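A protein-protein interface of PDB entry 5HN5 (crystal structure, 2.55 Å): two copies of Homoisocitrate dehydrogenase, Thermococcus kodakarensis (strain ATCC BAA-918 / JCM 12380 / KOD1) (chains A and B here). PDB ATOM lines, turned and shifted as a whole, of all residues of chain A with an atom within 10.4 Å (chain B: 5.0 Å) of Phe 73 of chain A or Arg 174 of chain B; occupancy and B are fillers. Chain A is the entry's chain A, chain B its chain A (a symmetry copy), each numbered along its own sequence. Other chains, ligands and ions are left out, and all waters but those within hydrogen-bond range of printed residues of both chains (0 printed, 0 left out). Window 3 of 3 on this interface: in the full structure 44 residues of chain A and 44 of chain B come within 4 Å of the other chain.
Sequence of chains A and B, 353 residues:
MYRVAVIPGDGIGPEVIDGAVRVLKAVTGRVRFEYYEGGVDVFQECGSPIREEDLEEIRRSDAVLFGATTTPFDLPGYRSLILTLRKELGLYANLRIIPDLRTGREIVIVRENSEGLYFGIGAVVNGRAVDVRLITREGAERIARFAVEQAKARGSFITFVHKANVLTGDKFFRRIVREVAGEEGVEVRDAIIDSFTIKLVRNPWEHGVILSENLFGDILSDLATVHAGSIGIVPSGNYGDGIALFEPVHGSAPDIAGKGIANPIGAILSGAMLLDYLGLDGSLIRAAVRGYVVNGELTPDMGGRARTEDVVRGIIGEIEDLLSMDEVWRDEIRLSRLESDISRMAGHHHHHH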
ATOM      1  N   VAL A  40     -15.136  -6.242 -16.174  1.00  0.00           N
ATOM      2  CA  VAL A  40     -14.609  -7.571 -15.860  1.00  0.00           C
ATOM      3  C   VAL A  40     -14.262  -7.726 -14.377  1.00  0.00           C
ATOM      4  O   VAL A  40     -14.562  -8.757 -13.802  1.00  0.00           O
ATOM      5  CB  VAL A  40     -13.418  -8.001 -16.761  1.00  0.00           C
ATOM      6  CG1 VAL A  40     -13.757  -7.822 -18.244  1.00  0.00           C
ATOM      7  CG2 VAL A  40     -12.145  -7.261 -16.405  1.00  0.00           C
ATOM      8  N   THR A  69     -16.189   0.066 -22.063  1.00  0.00           N
ATOM      9  CA  THR A  69     -15.942  -1.170 -21.364  1.00  0.00           C
ATOM     10  C   THR A  69     -15.200  -2.132 -22.277  1.00  0.00           C
ATOM     11  O   THR A  69     -15.513  -2.256 -23.481  1.00  0.00           O
ATOM     12  CB  THR A  69     -17.290  -1.785 -20.924  1.00  0.00           C
ATOM     13  OG1 THR A  69     -17.053  -2.922 -20.108  1.00  0.00           O
ATOM     14  CG2 THR A  69     -18.176  -2.204 -22.127  1.00  0.00           C
ATOM     15  N   THR A  70     -14.187  -2.792 -21.730  1.00  0.00           N
ATOM     16  CA  THR A  70     -13.449  -3.772 -22.501  1.00  0.00           C
ATOM     17  C   THR A  70     -14.148  -5.130 -22.435  1.00  0.00           C
ATOM     18  O   THR A  70     -14.247  -5.711 -21.378  1.00  0.00           O
ATOM     19  CB  THR A  70     -11.992  -3.891 -22.005  1.00  0.00           C
ATOM     20  OG1 THR A  70     -11.339  -2.605 -22.116  1.00  0.00           O
ATOM     21  CG2 THR A  70     -11.230  -4.944 -22.858  1.00  0.00           C
ATOM     22  N   THR A  71     -14.631  -5.649 -23.554  1.00  0.00           N
ATOM     23  CA  THR A  71     -15.246  -6.969 -23.528  1.00  0.00           C
ATOM     24  C   THR A  71     -14.261  -7.987 -24.102  1.00  0.00           C
ATOM     25  O   THR A  71     -14.168  -8.118 -25.326  1.00  0.00           O
ATOM     26  CB  THR A  71     -16.599  -6.990 -24.275  1.00  0.00           C
ATOM     27  OG1 THR A  71     -17.572  -6.264 -23.499  1.00  0.00           O
ATOM     28  CG2 THR A  71     -17.096  -8.454 -24.496  1.00  0.00           C
ATOM     29  N   PRO A  72     -13.510  -8.691 -23.227  1.00  0.00           N
ATOM     30  CA  PRO A  72     -12.475  -9.588 -23.749  1.00  0.00           C
ATOM     31  C   PRO A  72     -13.114 -10.834 -24.351  1.00  0.00           C
ATOM     32  O   PRO A  72     -14.056 -11.406 -23.781  1.00  0.00           O
ATOM     33  CB  PRO A  72     -11.632  -9.912 -22.519  1.00  0.00           C
ATOM     34  CG  PRO A  72     -12.587  -9.817 -21.385  1.00  0.00           C
ATOM     35  CD  PRO A  72     -13.570  -8.738 -21.757  1.00  0.00           C
ATOM     36  N   PHE A  73     -12.618 -11.210 -25.520  1.00  0.00           N
ATOM     37  CA  PHE A  73     -13.176 -12.305 -26.312  1.00  0.00           C
ATOM     38  C   PHE A  73     -13.073 -13.676 -25.626  1.00  0.00           C
ATOM     39  O   PHE A  73     -13.929 -14.550 -25.805  1.00  0.00           O
ATOM     40  CB  PHE A  73     -12.452 -12.354 -27.660  1.00  0.00           C
ATOM     41  CG  PHE A  73     -12.586 -13.658 -28.357  1.00  0.00           C
ATOM     42  CD1 PHE A  73     -13.672 -13.900 -29.184  1.00  0.00           C
ATOM     43  CD2 PHE A  73     -11.638 -14.661 -28.163  1.00  0.00           C
ATOM     44  CE1 PHE A  73     -13.808 -15.120 -29.824  1.00  0.00           C
ATOM     45  CE2 PHE A  73     -11.768 -15.882 -28.796  1.00  0.00           C
ATOM     46  CZ  PHE A  73     -12.856 -16.111 -29.631  1.00  0.00           C
ATOM     47  N   ASP A  74     -12.014 -13.834 -24.839  1.00  0.00           N
ATOM     48  CA  ASP A  74     -11.596 -15.109 -24.280  1.00  0.00           C
ATOM     49  C   ASP A  74     -11.896 -15.201 -22.780  1.00  0.00           C
ATOM     50  O   ASP A  74     -11.081 -15.710 -22.012  1.00  0.00           O
ATOM     51  CB  ASP A  74     -10.087 -15.258 -24.509  1.00  0.00           C
ATOM     52  CG  ASP A  74      -9.270 -14.130 -23.834  1.00  0.00           C
ATOM     53  OD1 ASP A  74      -9.549 -12.926 -24.080  1.00  0.00           O
ATOM     54  OD2 ASP A  74      -8.348 -14.452 -23.046  1.00  0.00           O
ATOM     55  N   LEU A  75     -13.057 -14.710 -22.355  1.00  0.00           N
ATOM     56  CA  LEU A  75     -13.422 -14.772 -20.950  1.00  0.00           C
ATOM     57  C   LEU A  75     -14.773 -15.440 -20.841  1.00  0.00           C
ATOM     58  O   LEU A  75     -15.799 -14.806 -21.035  1.00  0.00           O
ATOM     59  CB  LEU A  75     -13.447 -13.383 -20.325  1.00  0.00           C
ATOM     60  CG  LEU A  75     -13.833 -13.294 -18.844  1.00  0.00           C
ATOM     61  CD1 LEU A  75     -12.789 -13.946 -17.950  1.00  0.00           C
ATOM     62  CD2 LEU A  75     -14.026 -11.841 -18.444  1.00  0.00           C
ATOM     63  N   PRO A  76     -14.773 -16.739 -20.525  1.00  0.00           N
ATOM     64  CA  PRO A  76     -15.992 -17.552 -20.543  1.00  0.00           C
ATOM     65  C   PRO A  76     -17.138 -16.985 -19.718  1.00  0.00           C
ATOM     66  O   PRO A  76     -16.921 -16.417 -18.668  1.00  0.00           O
ATOM     67  CB  PRO A  76     -15.524 -18.885 -19.949  1.00  0.00           C
ATOM     68  CG  PRO A  76     -14.063 -18.950 -20.285  1.00  0.00           C
ATOM     69  CD  PRO A  76     -13.563 -17.540 -20.229  1.00  0.00           C
ATOM     70  N   GLY A  77     -18.356 -17.147 -20.209  1.00  0.00           N
ATOM     71  CA  GLY A  77     -19.555 -16.672 -19.526  1.00  0.00           C
ATOM     72  C   GLY A  77     -19.685 -15.157 -19.373  1.00  0.00           C
ATOM     73  O   GLY A  77     -20.588 -14.686 -18.685  1.00  0.00           O
ATOM     74  N   TYR A  78     -18.802 -14.381 -19.994  1.00  0.00           N
ATOM     75  CA  TYR A  78     -18.810 -12.946 -19.761  1.00  0.00           C
ATOM     76  C   TYR A  78     -19.601 -12.285 -20.846  1.00  0.00           C
ATOM     77  O   TYR A  78     -19.310 -12.474 -22.017  1.00  0.00           O
ATOM     78  CB  TYR A  78     -17.405 -12.356 -19.777  1.00  0.00           C
ATOM     79  CG  TYR A  78     -17.430 -10.866 -19.597  1.00  0.00           C
ATOM     80  CD1 TYR A  78     -17.547 -10.310 -18.335  1.00  0.00           C
ATOM     81  CD2 TYR A  78     -17.378  -9.998 -20.693  1.00  0.00           C
ATOM     82  CE1 TYR A  78     -17.569  -8.935 -18.158  1.00  0.00           C
ATOM     83  CE2 TYR A  78     -17.406  -8.624 -20.528  1.00  0.00           C
ATOM     84  CZ  TYR A  78     -17.507  -8.097 -19.258  1.00  0.00           C
ATOM     85  OH  TYR A  78     -17.541  -6.738 -19.044  1.00  0.00           O
ATOM     86  N   ARG A  79     -20.587 -11.496 -20.463  1.00  0.00           N
ATOM     87  CA  ARG A  79     -21.310 -10.692 -21.437  1.00  0.00           C
ATOM     88  C   ARG A  79     -20.935  -9.207 -21.273  1.00  0.00           C
ATOM     89  O   ARG A  79     -20.715  -8.714 -20.156  1.00  0.00           O
ATOM     90  CB  ARG A  79     -22.815 -10.941 -21.305  1.00  0.00           C
ATOM     91  CG  ARG A  79     -23.614 -10.533 -22.537  1.00  0.00           C
ATOM     92  CD  ARG A  79     -24.816 -11.441 -22.804  1.00  0.00           C
ATOM     93  NE  ARG A  79     -25.286 -11.310 -24.189  1.00  0.00           N
ATOM     94  CZ  ARG A  79     -26.337 -10.594 -24.593  1.00  0.00           C
ATOM     95  NH1 ARG A  79     -27.088  -9.921 -23.724  1.00  0.00           N
ATOM     96  NH2 ARG A  79     -26.645 -10.561 -25.893  1.00  0.00           N
ATOM     97  N   SER A  80     -20.779  -8.533 -22.406  1.00  0.00           N
ATOM     98  CA  SER A  80     -20.589  -7.075 -22.483  1.00  0.00           C
ATOM     99  C   SER A  80     -21.438  -6.304 -21.474  1.00  0.00           C
ATOM    100  O   SER A  80     -22.650  -6.528 -21.350  1.00  0.00           O
ATOM    101  CB  SER A  80     -20.976  -6.604 -23.882  1.00  0.00           C
ATOM    102  OG  SER A  80     -20.793  -5.208 -24.073  1.00  0.00           O
ATOM    103  N   VAL A 124     -25.183 -24.427 -30.395  1.00  0.00           N
ATOM    104  CA  VAL A 124     -24.415 -25.346 -31.238  1.00  0.00           C
ATOM    105  C   VAL A 124     -24.905 -26.745 -30.911  1.00  0.00           C
ATOM    106  O   VAL A 124     -25.257 -27.010 -29.777  1.00  0.00           O
ATOM    107  CB  VAL A 124     -22.905 -25.258 -30.994  1.00  0.00           C
ATOM    108  CG1 VAL A 124     -22.134 -26.044 -32.061  1.00  0.00           C
ATOM    109  CG2 VAL A 124     -22.474 -23.816 -31.008  1.00  0.00           C
ATOM    110  N   ALA A 129     -24.119 -24.710 -35.857  1.00  0.00           N
ATOM    111  CA  ALA A 129     -24.279 -23.513 -35.042  1.00  0.00           C
ATOM    112  C   ALA A 129     -25.299 -22.584 -35.663  1.00  0.00           C
ATOM    113  O   ALA A 129     -25.333 -22.363 -36.861  1.00  0.00           O
ATOM    114  CB  ALA A 129     -22.949 -22.804 -34.878  1.00  0.00           C
ATOM    115  N   ASP A 131     -27.865 -18.913 -35.002  1.00  0.00           N
ATOM    116  CA  ASP A 131     -28.270 -17.695 -34.285  1.00  0.00           C
ATOM    117  C   ASP A 131     -29.546 -17.262 -34.930  1.00  0.00           C
ATOM    118  O   ASP A 131     -29.667 -17.285 -36.151  1.00  0.00           O
ATOM    119  CB  ASP A 131     -27.270 -16.554 -34.432  1.00  0.00           C
ATOM    120  CG  ASP A 131     -25.900 -16.874 -33.848  1.00  0.00           C
ATOM    121  OD1 ASP A 131     -25.678 -16.614 -32.644  1.00  0.00           O
ATOM    122  OD2 ASP A 131     -25.039 -17.353 -34.624  1.00  0.00           O
ATOM    123  N   PRO A 254      -7.963   0.333 -25.070  1.00  0.00           N
ATOM    124  CA  PRO A 254      -7.030   0.033 -23.975  1.00  0.00           C
ATOM    125  C   PRO A 254      -5.571   0.377 -24.287  1.00  0.00           C
ATOM    126  O   PRO A 254      -4.815   0.666 -23.369  1.00  0.00           O
ATOM    127  CB  PRO A 254      -7.187  -1.481 -23.763  1.00  0.00           C
ATOM    128  CG  PRO A 254      -8.433  -1.864 -24.464  1.00  0.00           C
ATOM    129  CD  PRO A 254      -8.591  -0.887 -25.598  1.00  0.00           C
ATOM    130  N   PHE B 160     -10.020 -12.929 -40.614  1.00  0.00           N
ATOM    131  CA  PHE B 160     -11.343 -13.476 -40.414  1.00  0.00           C
ATOM    132  C   PHE B 160     -12.234 -12.415 -39.765  1.00  0.00           C
ATOM    133  O   PHE B 160     -11.956 -11.977 -38.658  1.00  0.00           O
ATOM    134  CB  PHE B 160     -11.301 -14.743 -39.572  1.00  0.00           C
ATOM    135  CG  PHE B 160     -12.653 -15.288 -39.298  1.00  0.00           C
ATOM    136  CD1 PHE B 160     -13.474 -15.668 -40.351  1.00  0.00           C
ATOM    137  CD2 PHE B 160     -13.151 -15.341 -38.010  1.00  0.00           C
ATOM    138  CE1 PHE B 160     -14.760 -16.127 -40.116  1.00  0.00           C
ATOM    139  CE2 PHE B 160     -14.435 -15.788 -37.771  1.00  0.00           C
ATOM    140  CZ  PHE B 160     -15.240 -16.175 -38.824  1.00  0.00           C
ATOM    141  N   HIS B 162     -15.812 -11.006 -38.138  1.00  0.00           N
ATOM    142  CA  HIS B 162     -16.893 -11.622 -37.367  1.00  0.00           C
ATOM    143  C   HIS B 162     -17.492 -10.727 -36.264  1.00  0.00           C
ATOM    144  O   HIS B 162     -17.087  -9.593 -36.092  1.00  0.00           O
ATOM    145  CB  HIS B 162     -16.358 -12.877 -36.703  1.00  0.00           C
ATOM    146  CG  HIS B 162     -15.278 -12.615 -35.700  1.00  0.00           C
ATOM    147  ND1 HIS B 162     -13.941 -12.631 -36.033  1.00  0.00           N
ATOM    148  CD2 HIS B 162     -15.330 -12.344 -34.375  1.00  0.00           C
ATOM    149  CE1 HIS B 162     -13.219 -12.379 -34.957  1.00  0.00           C
ATOM    150  NE2 HIS B 162     -14.036 -12.214 -33.936  1.00  0.00           N
ATOM    151  N   ALA B 164     -18.205 -12.603 -33.171  1.00  0.00           N
ATOM    152  CA  ALA B 164     -18.159 -13.715 -32.227  1.00  0.00           C
ATOM    153  C   ALA B 164     -18.537 -13.355 -30.795  1.00  0.00           C
ATOM    154  O   ALA B 164     -19.021 -14.221 -30.066  1.00  0.00           O
ATOM    155  CB  ALA B 164     -16.800 -14.378 -32.259  1.00  0.00           C
ATOM    156  N   ASP B 170     -20.555 -17.418 -35.021  1.00  0.00           N
ATOM    157  CA  ASP B 170     -19.245 -16.855 -35.398  1.00  0.00           C
ATOM    158  C   ASP B 170     -18.144 -17.314 -34.462  1.00  0.00           C
ATOM    159  O   ASP B 170     -16.989 -17.425 -34.868  1.00  0.00           O
ATOM    160  CB  ASP B 170     -19.270 -15.338 -35.398  1.00  0.00           C
ATOM    161  CG  ASP B 170     -19.511 -14.750 -36.772  1.00  0.00           C
ATOM    162  OD1 ASP B 170     -19.550 -15.496 -37.789  1.00  0.00           O
ATOM    163  OD2 ASP B 170     -19.638 -13.509 -36.825  1.00  0.00           O
ATOM    164  N   LYS B 171     -18.490 -17.560 -33.212  1.00  0.00           N
ATOM    165  CA  LYS B 171     -17.561 -18.192 -32.282  1.00  0.00           C
ATOM    166  C   LYS B 171     -17.137 -19.558 -32.860  1.00  0.00           C
ATOM    167  O   LYS B 171     -15.950 -19.831 -33.021  1.00  0.00           O
ATOM    168  CB  LYS B 171     -18.212 -18.341 -30.901  1.00  0.00           C
ATOM    169  CG  LYS B 171     -17.321 -17.995 -29.725  1.00  0.00           C
ATOM    170  CD  LYS B 171     -18.131 -17.387 -28.578  1.00  0.00           C
ATOM    171  CE  LYS B 171     -17.393 -17.468 -27.242  1.00  0.00           C
ATOM    172  NZ  LYS B 171     -16.039 -16.840 -27.271  1.00  0.00           N
ATOM    173  N   PHE B 172     -18.123 -20.379 -33.213  1.00  0.00           N
ATOM    174  CA  PHE B 172     -17.902 -21.692 -33.848  1.00  0.00           C
ATOM    175  C   PHE B 172     -17.045 -21.591 -35.104  1.00  0.00           C
ATOM    176  O   PHE B 172     -16.122 -22.386 -35.311  1.00  0.00           O
ATOM    177  CB  PHE B 172     -19.267 -22.267 -34.202  1.00  0.00           C
ATOM    178  CG  PHE B 172     -19.238 -23.627 -34.823  1.00  0.00           C
ATOM    179  CD1 PHE B 172     -19.088 -24.757 -34.035  1.00  0.00           C
ATOM    180  CD2 PHE B 172     -19.465 -23.782 -36.173  1.00  0.00           C
ATOM    181  CE1 PHE B 172     -19.118 -26.021 -34.596  1.00  0.00           C
ATOM    182  CE2 PHE B 172     -19.497 -25.042 -36.740  1.00  0.00           C
ATOM    183  CZ  PHE B 172     -19.313 -26.164 -35.953  1.00  0.00           C
ATOM    184  N   PHE B 173     -17.364 -20.603 -35.934  1.00  0.00           N
ATOM    185  CA  PHE B 173     -16.763 -20.450 -37.246  1.00  0.00           C
ATOM    186  C   PHE B 173     -15.305 -20.056 -37.079  1.00  0.00           C
ATOM    187  O   PHE B 173     -14.436 -20.493 -37.827  1.00  0.00           O
ATOM    188  CB  PHE B 173     -17.546 -19.356 -37.998  1.00  0.00           C
ATOM    189  CG  PHE B 173     -17.262 -19.246 -39.477  1.00  0.00           C
ATOM    190  CD1 PHE B 173     -16.341 -20.048 -40.136  1.00  0.00           C
ATOM    191  CD2 PHE B 173     -17.942 -18.276 -40.225  1.00  0.00           C
ATOM    192  CE1 PHE B 173     -16.101 -19.885 -41.494  1.00  0.00           C
ATOM    193  CE2 PHE B 173     -17.719 -18.120 -41.581  1.00  0.00           C
ATOM    194  CZ  PHE B 173     -16.801 -18.930 -42.213  1.00  0.00           C
ATOM    195  N   ARG B 174     -15.055 -19.190 -36.106  1.00  0.00           N
ATOM    196  CA  ARG B 174     -13.711 -18.698 -35.813  1.00  0.00           C
ATOM    197  C   ARG B 174     -12.789 -19.862 -35.456  1.00  0.00           C
ATOM    198  O   ARG B 174     -11.706 -19.983 -36.007  1.00  0.00           O
ATOM    199  CB  ARG B 174     -13.766 -17.707 -34.651  1.00  0.00           C
ATOM    200  CG  ARG B 174     -12.442 -17.065 -34.311  1.00  0.00           C
ATOM    201  CD  ARG B 174     -12.625 -16.008 -33.246  1.00  0.00           C
ATOM    202  NE  ARG B 174     -11.348 -15.413 -32.880  1.00  0.00           N
ATOM    203  CZ  ARG B 174     -10.446 -15.983 -32.079  1.00  0.00           C
ATOM    204  NH1 ARG B 174      -9.304 -15.357 -31.840  1.00  0.00           N
ATOM    205  NH2 ARG B 174     -10.663 -17.175 -31.528  1.00  0.00           N
ATOM    206  N   ARG B 175     -13.256 -20.695 -34.528  1.00  0.00           N
ATOM    207  CA  ARG B 175     -12.575 -21.903 -34.073  1.00  0.00           C
ATOM    208  C   ARG B 175     -12.124 -22.726 -35.247  1.00  0.00           C
ATOM    209  O   ARG B 175     -10.964 -23.162 -35.335  1.00  0.00           O
ATOM    210  CB  ARG B 175     -13.535 -22.765 -33.243  1.00  0.00           C
ATOM    211  CG  ARG B 175     -13.193 -22.934 -31.773  1.00  0.00           C
ATOM    212  CD  ARG B 175     -13.365 -24.397 -31.368  1.00  0.00           C
ATOM    213  NE  ARG B 175     -14.743 -24.871 -31.553  1.00  0.00           N
ATOM    214  CZ  ARG B 175     -15.095 -26.111 -31.899  1.00  0.00           C
ATOM    215  NH1 ARG B 175     -14.184 -27.060 -32.131  1.00  0.00           N
ATOM    216  NH2 ARG B 175     -16.381 -26.401 -32.036  1.00  0.00           N
ATOM    217  N   ILE B 176     -13.052 -22.958 -36.160  1.00  0.00           N
ATOM    218  CA  ILE B 176     -12.750 -23.838 -37.256  1.00  0.00           C
ATOM    219  C   ILE B 176     -11.740 -23.179 -38.189  1.00  0.00           C
ATOM    220  O   ILE B 176     -10.783 -23.821 -38.617  1.00  0.00           O
ATOM    221  CB  ILE B 176     -14.024 -24.301 -37.973  1.00  0.00           C
ATOM    222  CG1 ILE B 176     -14.761 -25.297 -37.076  1.00  0.00           C
ATOM    223  CG2 ILE B 176     -13.688 -24.940 -39.311  1.00  0.00           C
ATOM    224  CD1 ILE B 176     -16.174 -25.613 -37.513  1.00  0.00           C
ATOM    225  N   VAL B 177     -11.931 -21.896 -38.482  1.00  0.00           N
ATOM    226  CA  VAL B 177     -10.992 -21.176 -39.344  1.00  0.00           C
ATOM    227  C   VAL B 177      -9.575 -21.199 -38.754  1.00  0.00           C
ATOM    228  O   VAL B 177      -8.610 -21.327 -39.485  1.00  0.00           O
ATOM    229  CB  VAL B 177     -11.494 -19.742 -39.630  1.00  0.00           C
ATOM    230  CG1 VAL B 177     -10.405 -18.856 -40.217  1.00  0.00           C
ATOM    231  CG2 VAL B 177     -12.678 -19.806 -40.571  1.00  0.00           C
ATOM    232  N   ARG B 178      -9.459 -21.128 -37.436  1.00  0.00           N
ATOM    233  CA  ARG B 178      -8.147 -21.113 -36.771  1.00  0.00           C
ATOM    234  C   ARG B 178      -7.442 -22.473 -36.785  1.00  0.00           C
ATOM    235  O   ARG B 178      -6.233 -22.536 -37.020  1.00  0.00           O
ATOM    236  CB  ARG B 178      -8.258 -20.518 -35.349  1.00  0.00           C
ATOM    237  CG  ARG B 178      -8.498 -19.002 -35.417  1.00  0.00           C
ATOM    238  CD  ARG B 178      -8.567 -18.272 -34.081  1.00  0.00           C
ATOM    239  NE  ARG B 178      -7.235 -17.855 -33.650  1.00  0.00           N
ATOM    240  CZ  ARG B 178      -6.528 -18.427 -32.678  1.00  0.00           C
ATOM    241  NH1 ARG B 178      -7.026 -19.440 -31.973  1.00  0.00           N
ATOM    242  NH2 ARG B 178      -5.314 -17.964 -32.403  1.00  0.00           N
ATOM    243  N   ASP B 190      -7.753 -11.554 -36.397  1.00  0.00           N
ATOM    244  CA  ASP B 190      -9.144 -11.232 -36.071  1.00  0.00           C
ATOM    245  C   ASP B 190      -9.511  -9.837 -36.551  1.00  0.00           C
ATOM    246  O   ASP B 190      -8.698  -8.927 -36.565  1.00  0.00           O
ATOM    247  CB  ASP B 190      -9.387 -11.292 -34.561  1.00  0.00           C
ATOM    248  CG  ASP B 190      -9.578 -12.697 -34.056  1.00  0.00           C
ATOM    249  OD1 ASP B 190     -10.547 -13.348 -34.454  1.00  0.00           O
ATOM    250  OD2 ASP B 190      -8.773 -13.177 -33.241  1.00  0.00           O
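O of Phe 73 of chain A lies within hydrogen-bond range of NZ of Lys 171 of chain B, at 3.4 Å.
NH1 of Arg 174 of chain B lies within salt-bridge range of OD2 of Asp 190 of chain B (2.6 Å).
Phe 73 of chain A touches Ala 164 of chain B. Phe 73 of chain A touches Arg 174 of chain B (CZ to NH2, 3.1 Å). Val 124 of chain A touches Phe 172 of chain B. CB of Phe 172 of chain B touches CB of Ala 129 of chain A (3.8 Å).
Of the printed residues of chain B, Phe 73 of chain A touches Ala 164 (3.9 Å), Lys 171 (3.4 Å) and Arg 174 (3.1 Å). Arg 174 of chain B touches just one residue of chain A: Phe 73. Of chain A, only Phe 73 (3.9 Å) comes within 4 Å of Ala 164 of chain B. Of chain A, only Phe 73 (3.4 Å) comes within 4 Å of Lys 171 of chain B. Printed residues of chain B within 4 Å of Val 124 of chain A: Phe 172 (3.9 Å). Printed residues of chain A within 4 Å of Phe 172 of chain B: Val 124 and Ala 129. Printed residues of chain B within 4 Å of Ala 129 of chain A: Phe 172. Gly 77 of chain A touches none of the printed residues of chain B. Arg 175 of chain B touches none of the printed residues of chain A. The nearest printed residue of chain B that does not touch Phe 73 of chain A is His 162 of chain B (5.0 Å). The nearest residue of chain A that does not touch Arg 174 of chain B is Asp 74 of chain A (7.3 Å).
Of the 17 printed residues of chain A, 3 touch a printed residue of chain B. Among the printed residues, 5 pairs touch across the chains.
No position is printed for both chains. Of the 5 pairs that touch across the chains among the printed residues, none has its exchanged pair printed and touching as well.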
